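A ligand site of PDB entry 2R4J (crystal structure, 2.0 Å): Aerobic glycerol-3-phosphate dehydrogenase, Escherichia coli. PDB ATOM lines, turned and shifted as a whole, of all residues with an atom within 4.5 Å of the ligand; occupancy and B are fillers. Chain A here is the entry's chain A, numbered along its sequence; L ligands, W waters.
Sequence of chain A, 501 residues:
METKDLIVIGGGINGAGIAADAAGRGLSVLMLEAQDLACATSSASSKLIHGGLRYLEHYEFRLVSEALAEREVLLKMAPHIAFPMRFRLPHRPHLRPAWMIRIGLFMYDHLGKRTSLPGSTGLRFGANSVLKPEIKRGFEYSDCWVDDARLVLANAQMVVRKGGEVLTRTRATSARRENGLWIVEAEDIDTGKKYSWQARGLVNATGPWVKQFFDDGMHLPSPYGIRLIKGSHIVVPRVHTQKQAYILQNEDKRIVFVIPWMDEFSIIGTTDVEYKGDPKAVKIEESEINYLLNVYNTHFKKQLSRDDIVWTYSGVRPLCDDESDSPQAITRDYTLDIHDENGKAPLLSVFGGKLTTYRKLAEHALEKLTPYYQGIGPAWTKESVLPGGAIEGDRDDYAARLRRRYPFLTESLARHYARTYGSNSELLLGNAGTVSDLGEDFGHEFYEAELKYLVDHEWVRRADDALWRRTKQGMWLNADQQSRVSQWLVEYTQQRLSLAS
NH2 of Arg 254 lies within salt-bridge range of OD2 of Asp 272 (3.4 Å).
The side-chain hydroxyl (OH) of Tyr 55 is in hydrogen-bond range of the side-chain amino group (NZ) of Lys 354 (2.8 Å).
O of Thr 270 lies within hydrogen-bond range of NH2 of Arg 254, at 3.0 Å.
The side-chain carboxylate (OD1) of Asp 272 is in salt-bridge range of the guanidinium group (NH1) of Arg 317, 3.3 Å away.
NH2 of Arg 332 lies within salt-bridge range of OD1 of Asp 272 (2.8 Å).
O of Ile 255 is in hydrogen-bond range of O6 of the ligand.
NH2 of Arg 254 sits at hydrogen-bond distance from O6 of the ligand (3.1 Å).
O1 of the ligand is in salt-bridge range of NE of Arg 54, at 3.5 Å.
N of Ile 255 lies within hydrogen-bond range of O5 of the ligand, at 3.3 Å.
An oxygen (O2) of the ligand is in salt-bridge range of the guanidinium group of Arg 332 (3.1 Å).
An oxygen (O1) of the ligand is in hydrogen-bond range of the side-chain hydroxyl (OH) of Tyr 55, at 2.6 Å.
The guanidinium group (NH2) of Arg 317 lies within salt-bridge range of an oxygen (O3) of the ligand, at 2.6 Å.
The backbone NH of Thr 270 is in hydrogen-bond range of an oxygen (O6) of the ligand (3.2 Å).
Merely in contact with the ligand: Asp 272.
Hydrophobic or aromatic side chains that line the ligand: Tyr 55 and Ile 255.
Within 4 Å of the ligand: Arg 54, Tyr 55, Arg 254, Ile 255, Thr 270, Asp 272, Arg 317 and Arg 332.
The nearest printed residue that does not touch the ligand is Gly 269 (4.1 Å).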
ATOM      1  N   ARG A  54     -12.685  25.642 -19.239  1.00  0.00           N
ATOM      2  CA  ARG A  54     -13.900  25.483 -20.067  1.00  0.00           C
ATOM      3  C   ARG A  54     -14.993  24.539 -19.524  1.00  0.00           C
ATOM      4  O   ARG A  54     -16.143  24.604 -19.984  1.00  0.00           O
ATOM      5  CB  ARG A  54     -13.557  25.191 -21.541  1.00  0.00           C
ATOM      6  CG  ARG A  54     -13.000  23.818 -21.812  1.00  0.00           C
ATOM      7  CD  ARG A  54     -12.880  23.625 -23.324  1.00  0.00           C
ATOM      8  NE  ARG A  54     -12.822  22.206 -23.621  1.00  0.00           N
ATOM      9  CZ  ARG A  54     -13.886  21.433 -23.846  1.00  0.00           C
ATOM     10  NH1 ARG A  54     -15.104  21.957 -23.829  1.00  0.00           N
ATOM     11  NH2 ARG A  54     -13.730  20.141 -24.101  1.00  0.00           N
ATOM     12  N   TYR A  55     -14.638  23.659 -18.580  1.00  0.00           N
ATOM     13  CA  TYR A  55     -15.550  22.684 -18.032  1.00  0.00           C
ATOM     14  C   TYR A  55     -16.580  23.264 -17.037  1.00  0.00           C
ATOM     15  O   TYR A  55     -17.551  22.590 -16.710  1.00  0.00           O
ATOM     16  CB  TYR A  55     -14.815  21.549 -17.336  1.00  0.00           C
ATOM     17  CG  TYR A  55     -13.695  20.932 -18.133  1.00  0.00           C
ATOM     18  CD1 TYR A  55     -13.694  20.983 -19.530  1.00  0.00           C
ATOM     19  CD2 TYR A  55     -12.663  20.251 -17.494  1.00  0.00           C
ATOM     20  CE1 TYR A  55     -12.675  20.399 -20.268  1.00  0.00           C
ATOM     21  CE2 TYR A  55     -11.639  19.685 -18.220  1.00  0.00           C
ATOM     22  CZ  TYR A  55     -11.649  19.762 -19.602  1.00  0.00           C
ATOM     23  OH  TYR A  55     -10.609  19.187 -20.329  1.00  0.00           O
ATOM     24  N   ARG A 254     -15.147  26.557 -28.523  1.00  0.00           N
ATOM     25  CA  ARG A 254     -14.031  25.782 -28.022  1.00  0.00           C
ATOM     26  C   ARG A 254     -12.807  26.712 -27.972  1.00  0.00           C
ATOM     27  O   ARG A 254     -12.659  27.569 -28.837  1.00  0.00           O
ATOM     28  CB  ARG A 254     -13.739  24.589 -28.936  1.00  0.00           C
ATOM     29  CG  ARG A 254     -14.628  23.386 -28.672  1.00  0.00           C
ATOM     30  CD  ARG A 254     -14.186  22.186 -29.494  1.00  0.00           C
ATOM     31  NE  ARG A 254     -12.852  21.729 -29.124  1.00  0.00           N
ATOM     32  CZ  ARG A 254     -11.727  22.214 -29.628  1.00  0.00           C
ATOM     33  NH1 ARG A 254     -11.767  23.194 -30.529  1.00  0.00           N
ATOM     34  NH2 ARG A 254     -10.550  21.738 -29.225  1.00  0.00           N
ATOM     35  N   ILE A 255     -11.962  26.540 -26.971  1.00  0.00           N
ATOM     36  CA  ILE A 255     -10.846  27.461 -26.795  1.00  0.00           C
ATOM     37  C   ILE A 255      -9.632  26.700 -27.388  1.00  0.00           C
ATOM     38  O   ILE A 255      -9.596  25.462 -27.453  1.00  0.00           O
ATOM     39  CB  ILE A 255     -10.655  27.892 -25.310  1.00  0.00           C
ATOM     40  CG1 ILE A 255     -11.067  26.792 -24.382  1.00  0.00           C
ATOM     41  CG2 ILE A 255     -11.649  29.031 -24.868  1.00  0.00           C
ATOM     42  CD1 ILE A 255      -9.864  26.089 -23.699  1.00  0.00           C
ATOM     43  N   VAL A 256      -8.685  27.465 -27.924  1.00  0.00           N
ATOM     44  CA  VAL A 256      -7.494  26.924 -28.524  1.00  0.00           C
ATOM     45  C   VAL A 256      -6.322  27.626 -27.807  1.00  0.00           C
ATOM     46  O   VAL A 256      -6.403  28.806 -27.531  1.00  0.00           O
ATOM     47  CB  VAL A 256      -7.564  27.205 -29.980  1.00  0.00           C
ATOM     48  CG1 VAL A 256      -6.229  26.969 -30.659  1.00  0.00           C
ATOM     49  CG2 VAL A 256      -8.720  26.322 -30.649  1.00  0.00           C
ATOM     50  N   PHE A 257      -5.261  26.872 -27.471  1.00  0.00           N
ATOM     51  CA  PHE A 257      -4.020  27.447 -26.826  1.00  0.00           C
ATOM     52  C   PHE A 257      -2.886  27.722 -27.749  1.00  0.00           C
ATOM     53  O   PHE A 257      -2.694  26.967 -28.727  1.00  0.00           O
ATOM     54  CB  PHE A 257      -3.475  26.459 -25.790  1.00  0.00           C
ATOM     55  CG  PHE A 257      -4.484  26.114 -24.720  1.00  0.00           C
ATOM     56  CD1 PHE A 257      -4.793  27.019 -23.731  1.00  0.00           C
ATOM     57  CD2 PHE A 257      -5.100  24.850 -24.693  1.00  0.00           C
ATOM     58  CE1 PHE A 257      -5.689  26.731 -22.729  1.00  0.00           C
ATOM     59  CE2 PHE A 257      -6.025  24.550 -23.666  1.00  0.00           C
ATOM     60  CZ  PHE A 257      -6.323  25.489 -22.681  1.00  0.00           C
ATOM     61  N   GLY A 269      -2.923  24.338 -30.299  1.00  0.00           N
ATOM     62  CA  GLY A 269      -3.784  23.133 -30.226  1.00  0.00           C
ATOM     63  C   GLY A 269      -4.929  23.516 -29.325  1.00  0.00           C
ATOM     64  O   GLY A 269      -4.823  24.506 -28.582  1.00  0.00           O
ATOM     65  N   THR A 270      -6.014  22.744 -29.351  1.00  0.00           N
ATOM     66  CA  THR A 270      -6.100  21.489 -30.077  1.00  0.00           C
ATOM     67  C   THR A 270      -7.516  21.518 -30.670  1.00  0.00           C
ATOM     68  O   THR A 270      -8.113  22.613 -30.825  1.00  0.00           O
ATOM     69  CB  THR A 270      -5.784  20.339 -29.091  1.00  0.00           C
ATOM     70  OG1 THR A 270      -5.796  19.087 -29.762  1.00  0.00           O
ATOM     71  CG2 THR A 270      -6.813  20.302 -28.003  1.00  0.00           C
ATOM     72  N   ASP A 272     -11.214  18.839 -31.695  1.00  0.00           N
ATOM     73  CA  ASP A 272     -12.108  17.742 -31.118  1.00  0.00           C
ATOM     74  C   ASP A 272     -12.774  16.972 -32.236  1.00  0.00           C
ATOM     75  O   ASP A 272     -13.794  17.407 -32.682  1.00  0.00           O
ATOM     76  CB  ASP A 272     -13.237  18.366 -30.312  1.00  0.00           C
ATOM     77  CG  ASP A 272     -12.943  18.508 -28.837  1.00  0.00           C
ATOM     78  OD1 ASP A 272     -12.603  17.467 -28.239  1.00  0.00           O
ATOM     79  OD2 ASP A 272     -13.092  19.647 -28.244  1.00  0.00           O
ATOM     80  N   ARG A 317      -8.358  11.192 -27.430  1.00  0.00           N
ATOM     81  CA  ARG A 317      -8.793  11.123 -26.018  1.00  0.00           C
ATOM     82  C   ARG A 317      -9.720   9.909 -25.803  1.00  0.00           C
ATOM     83  O   ARG A 317     -10.772   9.796 -26.469  1.00  0.00           O
ATOM     84  CB  ARG A 317      -9.554  12.393 -25.631  1.00  0.00           C
ATOM     85  CG  ARG A 317      -8.851  13.726 -25.989  1.00  0.00           C
ATOM     86  CD  ARG A 317      -9.813  14.831 -25.733  1.00  0.00           C
ATOM     87  NE  ARG A 317      -9.343  16.191 -25.966  1.00  0.00           N
ATOM     88  CZ  ARG A 317      -9.288  16.809 -27.159  1.00  0.00           C
ATOM     89  NH1 ARG A 317      -9.563  16.182 -28.270  1.00  0.00           N
ATOM     90  NH2 ARG A 317      -8.985  18.100 -27.234  1.00  0.00           N
ATOM     91  N   ARG A 332     -14.824  15.139 -19.358  1.00  0.00           N
ATOM     92  CA  ARG A 332     -13.438  14.748 -19.217  1.00  0.00           C
ATOM     93  C   ARG A 332     -13.176  14.133 -17.864  1.00  0.00           C
ATOM     94  O   ARG A 332     -12.058  13.732 -17.558  1.00  0.00           O
ATOM     95  CB  ARG A 332     -12.520  15.948 -19.497  1.00  0.00           C
ATOM     96  CG  ARG A 332     -12.048  16.053 -20.978  1.00  0.00           C
ATOM     97  CD  ARG A 332     -13.193  16.513 -21.910  1.00  0.00           C
ATOM     98  NE  ARG A 332     -12.721  16.966 -23.218  1.00  0.00           N
ATOM     99  CZ  ARG A 332     -13.415  16.940 -24.340  1.00  0.00           C
ATOM    100  NH1 ARG A 332     -14.663  16.479 -24.351  1.00  0.00           N
ATOM    101  NH2 ARG A 332     -12.872  17.396 -25.453  1.00  0.00           N
ATOM    102  N   LYS A 354      -7.869  12.692 -17.359  1.00  0.00           N
ATOM    103  CA  LYS A 354      -6.808  13.645 -17.664  1.00  0.00           C
ATOM    104  C   LYS A 354      -5.401  13.365 -17.081  1.00  0.00           C
ATOM    105  O   LYS A 354      -5.224  12.654 -16.108  1.00  0.00           O
ATOM    106  CB  LYS A 354      -7.251  15.051 -17.245  1.00  0.00           C
ATOM    107  CG  LYS A 354      -8.514  15.593 -17.942  1.00  0.00           C
ATOM    108  CD  LYS A 354      -8.806  16.988 -17.528  1.00  0.00           C
ATOM    109  CE  LYS A 354      -7.903  18.087 -18.142  1.00  0.00           C
ATOM    110  NZ  LYS A 354      -8.015  18.437 -19.600  1.00  0.00           N
HETATM  111  P1  LIG L   1      -9.824  19.254 -23.970  1.00  0.00           P
HETATM  112  O1  LIG L   1     -10.177  20.041 -22.782  1.00  0.00           O
HETATM  113  O2  LIG L   1      -9.689  17.698 -23.633  1.00  0.00           O
HETATM  114  O3  LIG L   1      -8.990  19.686 -25.123  1.00  0.00           O
HETATM  115  O4  LIG L   1     -11.072  19.879 -24.900  1.00  0.00           O
HETATM  116  C1  LIG L   1     -11.132  20.825 -26.079  1.00  0.00           C
HETATM  117  C2  LIG L   1     -10.649  22.355 -26.030  1.00  0.00           C
HETATM  118  O5  LIG L   1     -11.504  23.362 -26.140  1.00  0.00           O
HETATM  119  C3  LIG L   1      -9.068  22.609 -25.995  1.00  0.00           C
HETATM  120  O6  LIG L   1      -8.427  23.024 -27.316  1.00  0.00           O
HETATM  121  O   HOH W   1      -9.453  22.656 -21.934  1.00  0.00           O
HETATM  122  O   HOH W   2      -6.003  20.402 -24.383  1.00  0.00           O
